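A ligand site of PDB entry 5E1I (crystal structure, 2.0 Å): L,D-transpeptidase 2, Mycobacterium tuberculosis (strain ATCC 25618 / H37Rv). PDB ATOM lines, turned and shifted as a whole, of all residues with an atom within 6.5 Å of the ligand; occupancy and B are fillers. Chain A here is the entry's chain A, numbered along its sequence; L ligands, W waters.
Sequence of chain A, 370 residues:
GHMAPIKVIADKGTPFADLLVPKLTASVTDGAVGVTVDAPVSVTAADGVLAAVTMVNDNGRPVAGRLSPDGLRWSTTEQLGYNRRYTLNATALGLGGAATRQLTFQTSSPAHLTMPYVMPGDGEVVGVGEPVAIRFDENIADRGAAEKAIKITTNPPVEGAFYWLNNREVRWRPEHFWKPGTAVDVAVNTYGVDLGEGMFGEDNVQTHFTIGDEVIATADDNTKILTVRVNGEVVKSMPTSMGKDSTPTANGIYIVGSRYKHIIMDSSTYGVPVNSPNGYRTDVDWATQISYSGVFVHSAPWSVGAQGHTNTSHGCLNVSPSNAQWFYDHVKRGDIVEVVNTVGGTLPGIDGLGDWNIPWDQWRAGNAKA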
ATOM      1  N   SER A 241     -21.548  11.646 -26.453  1.00  0.00           N
ATOM      2  CA  SER A 241     -20.461  10.908 -27.069  1.00  0.00           C
ATOM      3  C   SER A 241     -19.892  10.014 -25.996  1.00  0.00           C
ATOM      4  O   SER A 241     -19.329  10.492 -25.022  1.00  0.00           O
ATOM      5  CB  SER A 241     -19.383  11.850 -27.631  1.00  0.00           C
ATOM      6  OG  SER A 241     -18.399  11.116 -28.365  1.00  0.00           O
ATOM      7  N   GLY A 243     -17.812   6.119 -24.971  1.00  0.00           N
ATOM      8  CA  GLY A 243     -16.475   5.580 -25.137  1.00  0.00           C
ATOM      9  C   GLY A 243     -16.205   5.112 -26.538  1.00  0.00           C
ATOM     10  O   GLY A 243     -16.999   4.372 -27.123  1.00  0.00           O
ATOM     11  N   MET A 265     -10.156  15.160 -13.014  1.00  0.00           N
ATOM     12  CA  MET A 265     -10.126  13.732 -13.314  1.00  0.00           C
ATOM     13  C   MET A 265      -8.716  13.206 -13.337  1.00  0.00           C
ATOM     14  O   MET A 265      -7.944  13.566 -14.198  1.00  0.00           O
ATOM     15  CB  MET A 265     -10.777  13.448 -14.652  1.00  0.00           C
ATOM     16  CG  MET A 265     -12.144  13.973 -14.773  1.00  0.00           C
ATOM     17  SD  MET A 265     -13.287  13.057 -13.753  1.00  0.00           S
ATOM     18  CE  MET A 265     -14.722  13.307 -14.802  1.00  0.00           C
ATOM     19  N   ASP A 266      -8.393  12.313 -12.407  1.00  0.00           N
ATOM     20  CA  ASP A 266      -7.057  11.772 -12.324  1.00  0.00           C
ATOM     21  C   ASP A 266      -7.120  10.271 -12.590  1.00  0.00           C
ATOM     22  O   ASP A 266      -7.680   9.530 -11.790  1.00  0.00           O
ATOM     23  CB  ASP A 266      -6.455  12.059 -10.942  1.00  0.00           C
ATOM     24  CG  ASP A 266      -4.950  11.828 -10.885  1.00  0.00           C
ATOM     25  OD1 ASP A 266      -4.454  10.877 -11.526  1.00  0.00           O
ATOM     26  OD2 ASP A 266      -4.280  12.599 -10.174  1.00  0.00           O
ATOM     27  N   TYR A 270      -8.069   5.764 -10.650  1.00  0.00           N
ATOM     28  CA  TYR A 270      -8.675   4.535 -11.165  1.00  0.00           C
ATOM     29  C   TYR A 270      -7.618   3.576 -11.708  1.00  0.00           C
ATOM     30  O   TYR A 270      -7.899   2.789 -12.605  1.00  0.00           O
ATOM     31  CB  TYR A 270      -9.697   4.880 -12.243  1.00  0.00           C
ATOM     32  CG  TYR A 270     -10.590   5.992 -11.807  1.00  0.00           C
ATOM     33  CD1 TYR A 270     -11.432   5.834 -10.717  1.00  0.00           C
ATOM     34  CD2 TYR A 270     -10.570   7.225 -12.446  1.00  0.00           C
ATOM     35  CE1 TYR A 270     -12.252   6.860 -10.280  1.00  0.00           C
ATOM     36  CE2 TYR A 270     -11.393   8.261 -12.027  1.00  0.00           C
ATOM     37  CZ  TYR A 270     -12.229   8.079 -10.938  1.00  0.00           C
ATOM     38  OH  TYR A 270     -13.043   9.099 -10.506  1.00  0.00           O
ATOM     39  N   TYR A 280      -4.560  10.212 -17.939  1.00  0.00           N
ATOM     40  CA  TYR A 280      -5.070  11.566 -18.134  1.00  0.00           C
ATOM     41  C   TYR A 280      -5.140  12.296 -16.801  1.00  0.00           C
ATOM     42  O   TYR A 280      -5.192  11.660 -15.745  1.00  0.00           O
ATOM     43  CB  TYR A 280      -6.466  11.538 -18.775  1.00  0.00           C
ATOM     44  CG  TYR A 280      -7.402  10.565 -18.069  1.00  0.00           C
ATOM     45  CD1 TYR A 280      -8.020  10.899 -16.874  1.00  0.00           C
ATOM     46  CD2 TYR A 280      -7.639   9.299 -18.606  1.00  0.00           C
ATOM     47  CE1 TYR A 280      -8.860  10.022 -16.236  1.00  0.00           C
ATOM     48  CE2 TYR A 280      -8.487   8.416 -17.969  1.00  0.00           C
ATOM     49  CZ  TYR A 280      -9.092   8.771 -16.789  1.00  0.00           C
ATOM     50  OH  TYR A 280      -9.931   7.889 -16.142  1.00  0.00           O
ATOM     51  N   ARG A 281      -5.123  13.621 -16.846  1.00  0.00           N
ATOM     52  CA  ARG A 281      -5.393  14.433 -15.676  1.00  0.00           C
ATOM     53  C   ARG A 281      -5.985  15.741 -16.154  1.00  0.00           C
ATOM     54  O   ARG A 281      -5.250  16.656 -16.540  1.00  0.00           O
ATOM     55  CB  ARG A 281      -4.119  14.664 -14.854  1.00  0.00           C
ATOM     56  CG  ARG A 281      -4.366  15.425 -13.555  1.00  0.00           C
ATOM     57  CD  ARG A 281      -3.052  15.641 -12.814  1.00  0.00           C
ATOM     58  NE  ARG A 281      -1.986  15.889 -13.792  1.00  0.00           N
ATOM     59  CZ  ARG A 281      -0.820  15.264 -13.804  1.00  0.00           C
ATOM     60  NH1 ARG A 281      -0.510  14.367 -12.863  1.00  0.00           N
ATOM     61  NH2 ARG A 281       0.054  15.560 -14.748  1.00  0.00           N
ATOM     62  N   THR A 282      -7.309  15.805 -16.145  1.00  0.00           N
ATOM     63  CA  THR A 282      -8.019  16.930 -16.745  1.00  0.00           C
ATOM     64  C   THR A 282      -9.114  17.473 -15.843  1.00  0.00           C
ATOM     65  O   THR A 282      -9.825  16.722 -15.183  1.00  0.00           O
ATOM     66  CB  THR A 282      -8.652  16.520 -18.094  1.00  0.00           C
ATOM     67  OG1 THR A 282      -7.671  15.888 -18.922  1.00  0.00           O
ATOM     68  CG2 THR A 282      -9.198  17.748 -18.815  1.00  0.00           C
ATOM     69  N   VAL A 284     -12.665  19.119 -15.370  1.00  0.00           N
ATOM     70  CA  VAL A 284     -13.892  19.126 -16.157  1.00  0.00           C
ATOM     71  C   VAL A 284     -15.035  19.734 -15.372  1.00  0.00           C
ATOM     72  O   VAL A 284     -15.039  19.761 -14.140  1.00  0.00           O
ATOM     73  CB  VAL A 284     -14.306  17.720 -16.624  1.00  0.00           C
ATOM     74  CG1 VAL A 284     -13.193  17.074 -17.435  1.00  0.00           C
ATOM     75  CG2 VAL A 284     -14.652  16.844 -15.428  1.00  0.00           C
ATOM     76  N   SER A 293     -15.383   2.965 -11.117  1.00  0.00           N
ATOM     77  CA  SER A 293     -14.356   2.793 -12.135  1.00  0.00           C
ATOM     78  C   SER A 293     -14.097   4.073 -12.936  1.00  0.00           C
ATOM     79  O   SER A 293     -13.249   4.079 -13.833  1.00  0.00           O
ATOM     80  CB  SER A 293     -14.738   1.657 -13.082  1.00  0.00           C
ATOM     81  OG  SER A 293     -15.869   1.998 -13.870  1.00  0.00           O
ATOM     82  N   GLY A 294     -14.819   5.143 -12.640  1.00  0.00           N
ATOM     83  CA  GLY A 294     -14.532   6.447 -13.241  1.00  0.00           C
ATOM     84  C   GLY A 294     -15.429   6.944 -14.363  1.00  0.00           C
ATOM     85  O   GLY A 294     -15.080   7.896 -15.064  1.00  0.00           O
ATOM     86  N   VAL A 295     -16.590   6.321 -14.553  1.00  0.00           N
ATOM     87  CA  VAL A 295     -17.502   6.823 -15.568  1.00  0.00           C
ATOM     88  C   VAL A 295     -18.289   7.987 -14.985  1.00  0.00           C
ATOM     89  O   VAL A 295     -18.866   7.877 -13.890  1.00  0.00           O
ATOM     90  CB  VAL A 295     -18.480   5.727 -16.078  1.00  0.00           C
ATOM     91  CG1 VAL A 295     -19.495   6.320 -17.029  1.00  0.00           C
ATOM     92  CG2 VAL A 295     -17.708   4.624 -16.797  1.00  0.00           C
ATOM     93  N   PHE A 296     -18.265   9.120 -15.711  1.00  0.00           N
ATOM     94  CA  PHE A 296     -19.008  10.323 -15.354  1.00  0.00           C
ATOM     95  C   PHE A 296     -19.877  10.808 -16.510  1.00  0.00           C
ATOM     96  O   PHE A 296     -19.542  10.600 -17.684  1.00  0.00           O
ATOM     97  CB  PHE A 296     -18.074  11.487 -14.983  1.00  0.00           C
ATOM     98  CG  PHE A 296     -17.361  11.331 -13.678  1.00  0.00           C
ATOM     99  CD1 PHE A 296     -16.257  10.494 -13.562  1.00  0.00           C
ATOM    100  CD2 PHE A 296     -17.743  12.073 -12.572  1.00  0.00           C
ATOM    101  CE1 PHE A 296     -15.590  10.378 -12.354  1.00  0.00           C
ATOM    102  CE2 PHE A 296     -17.075  11.957 -11.364  1.00  0.00           C
ATOM    103  CZ  PHE A 296     -15.997  11.108 -11.262  1.00  0.00           C
ATOM    104  N   HIS A 298     -20.495  14.398 -17.850  1.00  0.00           N
ATOM    105  CA  HIS A 298     -19.867  15.695 -17.611  1.00  0.00           C
ATOM    106  C   HIS A 298     -19.823  16.602 -18.844  1.00  0.00           C
ATOM    107  O   HIS A 298     -20.114  16.168 -19.954  1.00  0.00           O
ATOM    108  CB  HIS A 298     -18.434  15.502 -17.102  1.00  0.00           C
ATOM    109  CG  HIS A 298     -17.497  14.956 -18.139  1.00  0.00           C
ATOM    110  ND1 HIS A 298     -16.809  15.768 -19.014  1.00  0.00           N
ATOM    111  CD2 HIS A 298     -17.162  13.683 -18.454  1.00  0.00           C
ATOM    112  CE1 HIS A 298     -16.081  15.015 -19.829  1.00  0.00           C
ATOM    113  NE2 HIS A 298     -16.276  13.751 -19.507  1.00  0.00           N
ATOM    114  N   ALA A 300     -18.361  18.491 -21.914  1.00  0.00           N
ATOM    115  CA  ALA A 300     -17.306  18.245 -22.873  1.00  0.00           C
ATOM    116  C   ALA A 300     -17.461  19.190 -24.065  1.00  0.00           C
ATOM    117  O   ALA A 300     -17.928  18.777 -25.124  1.00  0.00           O
ATOM    118  CB  ALA A 300     -17.321  16.820 -23.324  1.00  0.00           C
ATOM    119  N   TRP A 302     -15.322  20.226 -26.004  1.00  0.00           N
ATOM    120  CA  TRP A 302     -14.435  19.854 -27.102  1.00  0.00           C
ATOM    121  C   TRP A 302     -15.076  18.873 -28.063  1.00  0.00           C
ATOM    122  O   TRP A 302     -14.620  18.731 -29.201  1.00  0.00           O
ATOM    123  CB  TRP A 302     -13.121  19.283 -26.576  1.00  0.00           C
ATOM    124  CG  TRP A 302     -13.259  18.101 -25.675  1.00  0.00           C
ATOM    125  CD1 TRP A 302     -13.283  16.783 -26.034  1.00  0.00           C
ATOM    126  CD2 TRP A 302     -13.375  18.122 -24.246  1.00  0.00           C
ATOM    127  NE1 TRP A 302     -13.408  15.990 -24.923  1.00  0.00           N
ATOM    128  CE2 TRP A 302     -13.466  16.784 -23.809  1.00  0.00           C
ATOM    129  CE3 TRP A 302     -13.404  19.148 -23.289  1.00  0.00           C
ATOM    130  CZ2 TRP A 302     -13.606  16.448 -22.470  1.00  0.00           C
ATOM    131  CZ3 TRP A 302     -13.538  18.805 -21.955  1.00  0.00           C
ATOM    132  CH2 TRP A 302     -13.629  17.461 -21.555  1.00  0.00           C
ATOM    133  N   SER A 303     -16.133  18.184 -27.634  1.00  0.00           N
ATOM    134  CA  SER A 303     -16.712  17.136 -28.480  1.00  0.00           C
ATOM    135  C   SER A 303     -18.180  17.380 -28.821  1.00  0.00           C
ATOM    136  O   SER A 303     -18.881  16.463 -29.239  1.00  0.00           O
ATOM    137  CB  SER A 303     -16.569  15.768 -27.802  1.00  0.00           C
ATOM    138  OG  SER A 303     -17.091  15.795 -26.486  1.00  0.00           O
ATOM    139  N   THR A 312     -16.312   9.211 -28.836  1.00  0.00           N
ATOM    140  CA  THR A 312     -14.954   9.713 -28.808  1.00  0.00           C
ATOM    141  C   THR A 312     -14.273   9.721 -27.436  1.00  0.00           C
ATOM    142  O   THR A 312     -13.120  10.134 -27.318  1.00  0.00           O
ATOM    143  CB  THR A 312     -14.870  11.163 -29.357  1.00  0.00           C
ATOM    144  OG1 THR A 312     -15.660  12.032 -28.529  1.00  0.00           O
ATOM    145  CG2 THR A 312     -15.370  11.236 -30.796  1.00  0.00           C
ATOM    146  N   SER A 313     -14.960   9.288 -26.376  1.00  0.00           N
ATOM    147  CA  SER A 313     -14.403   9.438 -25.024  1.00  0.00           C
ATOM    148  C   SER A 313     -13.642   8.220 -24.527  1.00  0.00           C
ATOM    149  O   SER A 313     -13.565   7.204 -25.213  1.00  0.00           O
ATOM    150  CB  SER A 313     -15.507   9.753 -24.010  1.00  0.00           C
ATOM    151  OG  SER A 313     -16.149   8.569 -23.563  1.00  0.00           O
ATOM    152  N   HIS A 314     -13.100   8.344 -23.311  1.00  0.00           N
ATOM    153  CA  HIS A 314     -12.463   7.248 -22.582  1.00  0.00           C
ATOM    154  C   HIS A 314     -13.461   6.301 -21.909  1.00  0.00           C
ATOM    155  O   HIS A 314     -13.076   5.333 -21.255  1.00  0.00           O
ATOM    156  CB  HIS A 314     -11.508   7.798 -21.519  1.00  0.00           C
ATOM    157  CG  HIS A 314     -10.218   8.337 -22.064  1.00  0.00           C
ATOM    158  ND1 HIS A 314      -9.695   7.929 -23.270  1.00  0.00           N
ATOM    159  CD2 HIS A 314      -9.347   9.233 -21.548  1.00  0.00           C
ATOM    160  CE1 HIS A 314      -8.556   8.566 -23.489  1.00  0.00           C
ATOM    161  NE2 HIS A 314      -8.320   9.359 -22.458  1.00  0.00           N
ATOM    162  N   GLY A 315     -14.753   6.588 -22.040  1.00  0.00           N
ATOM    163  CA  GLY A 315     -15.783   5.783 -21.402  1.00  0.00           C
ATOM    164  C   GLY A 315     -16.870   6.660 -20.794  1.00  0.00           C
ATOM    165  O   GLY A 315     -18.017   6.244 -20.630  1.00  0.00           O
ATOM    166  N   CYS A 316     -16.489   7.893 -20.468  1.00  0.00           N
ATOM    167  CA  CYS A 316     -17.423   8.875 -19.933  1.00  0.00           C
ATOM    168  C   CYS A 316     -18.561   9.191 -20.894  1.00  0.00           C
ATOM    169  O   CYS A 316     -18.491   8.908 -22.098  1.00  0.00           O
ATOM    170  CB  CYS A 316     -16.695  10.177 -19.594  1.00  0.00           C
ATOM    171  SG  CYS A 316     -15.677  10.135 -18.109  1.00  0.00           S
ATOM    172  N   LEU A 317     -19.607   9.805 -20.349  1.00  0.00           N
ATOM    173  CA  LEU A 317     -20.727  10.242 -21.158  1.00  0.00           C
ATOM    174  C   LEU A 317     -20.569  11.738 -21.388  1.00  0.00           C
ATOM    175  O   LEU A 317     -21.015  12.558 -20.596  1.00  0.00           O
ATOM    176  CB  LEU A 317     -22.064   9.906 -20.490  1.00  0.00           C
ATOM    177  CG  LEU A 317     -22.616   8.500 -20.775  1.00  0.00           C
ATOM    178  CD1 LEU A 317     -21.594   7.404 -20.507  1.00  0.00           C
ATOM    179  CD2 LEU A 317     -23.899   8.201 -19.959  1.00  0.00           C
ATOM    180  N   ASN A 318     -19.880  12.072 -22.476  1.00  0.00           N
ATOM    181  CA  ASN A 318     -19.695  13.445 -22.888  1.00  0.00           C
ATOM    182  C   ASN A 318     -21.029  14.073 -23.279  1.00  0.00           C
ATOM    183  O   ASN A 318     -21.711  13.537 -24.140  1.00  0.00           O
ATOM    184  CB  ASN A 318     -18.734  13.536 -24.077  1.00  0.00           C
ATOM    185  CG  ASN A 318     -17.269  13.466 -23.669  1.00  0.00           C
ATOM    186  OD1 ASN A 318     -16.390  13.908 -24.424  1.00  0.00           O
ATOM    187  ND2 ASN A 318     -17.004  12.915 -22.506  1.00  0.00           N
HETATM  188  O1  LIG L   1     -14.399  12.239 -22.642  1.00  0.00           O
HETATM  189  C1  LIG L   1     -13.231  12.601 -22.360  1.00  0.00           C
HETATM  190  O2  LIG L   1     -12.341  13.051 -23.136  1.00  0.00           O
HETATM  191  C2  LIG L   1     -12.854  12.466 -20.899  1.00  0.00           C
HETATM  192  C3  LIG L   1     -11.693  13.201 -20.319  1.00  0.00           C
HETATM  193  S1  LIG L   1     -10.164  12.602 -21.128  1.00  0.00           S
HETATM  194  C4  LIG L   1      -9.653  14.130 -21.956  1.00  0.00           C
HETATM  195  C5  LIG L   1     -11.858  12.796 -18.864  1.00  0.00           C
HETATM  196  C6  LIG L   1     -10.533  12.436 -18.219  1.00  0.00           C
HETATM  197  C7  LIG L   1     -13.029  11.795 -18.783  1.00  0.00           C
HETATM  198  N1  LIG L   1     -13.721  11.987 -20.072  1.00  0.00           N
HETATM  199  C8  LIG L   1     -12.850  10.251 -18.621  1.00  0.00           C
HETATM  200  C9  LIG L   1     -14.100   9.555 -19.154  1.00  0.00           C
HETATM  201  O3  LIG L   1     -14.172   9.081 -20.275  1.00  0.00           O
HETATM  202  C10 LIG L   1     -12.485   9.595 -17.280  1.00  0.00           C
HETATM  203  O4  LIG L   1     -13.151   8.324 -17.249  1.00  0.00           O
HETATM  204  C11 LIG L   1     -12.771  10.361 -15.995  1.00  0.00           C
HETATM  205  O   HOH W   1     -13.489  13.480 -25.447  1.00  0.00           O
HETATM  206  O   HOH W   2      -6.418  14.207 -22.077  1.00  0.00           O
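The side-chain hydroxyl (OH) of Tyr 280 sits close to an oxygen (O4) of the ligand (3.4 Å).
C9 of the ligand is covalently linked to SG of Cys 316, at 2.0 Å.
An oxygen (O1) of the ligand is in hydrogen-bond range of the side-chain amide nitrogen (ND2) of Asn 318 (2.7 Å).
N of Cys 316 sits at hydrogen-bond distance from O3 of the ligand.
A nitrogen (N1) of the ligand is in hydrogen-bond range of a ring nitrogen (NE2) of His 298.
The backbone NH (N) of Gly 315 is in hydrogen-bond range of an oxygen (O3) of the ligand (3.1 Å).
O3 of the ligand sits close to N of His 314 (3.3 Å).
O4 of the ligand sits at hydrogen-bond distance from O of Gly 294, 2.9 Å away.
The side-chain hydroxyl of Ser 313 lies within hydrogen-bond range of the backbone NH of Gly 243, 3.3 Å away.
N of His 298 lies within hydrogen-bond range of O of Leu 317, at 3.3 Å.
SG of Cys 316 sits at hydrogen-bond distance from N of Phe 296 (3.7 Å).
The side-chain hydroxyl (OG) of Ser 303 lies within hydrogen-bond range of the side-chain amide oxygen (OD1) of Asn 318 (2.9 Å).
The backbone NH (N) of Met 265 sits at hydrogen-bond distance from the backbone carbonyl oxygen (O) of Thr 282 (2.7 Å).
The backbone NH of Ser 241 sits at hydrogen-bond distance from the backbone carbonyl oxygen of Asn 318 (3.0 Å).
The side-chain hydroxyl (OG) of Ser 313 lies within hydrogen-bond range of the backbone carbonyl oxygen (O) of Cys 316, 2.8 Å away.
The side-chain amide nitrogen (ND2) of Asn 318 is in hydrogen-bond range of a ring nitrogen (NE2) of His 298.
Met 265 touches the ligand (SD to C11, 3.5 Å).
Trp 302 touches the ligand.
Ser 313 touches the ligand.
Hydrophobic or aromatic side chains within 4 Å of the ligand: Met 265, Tyr 280, His 298, Trp 302 and His 314.
The nearest printed residue that does not touch the ligand is Thr 282 (4.03 Å).
Water W1 lies within hydrogen-bond range of NE1 of Trp 302 (2.6 Å), O2 of the ligand (2.6 Å) and OD1 of Asn 318 (3.1 Å).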
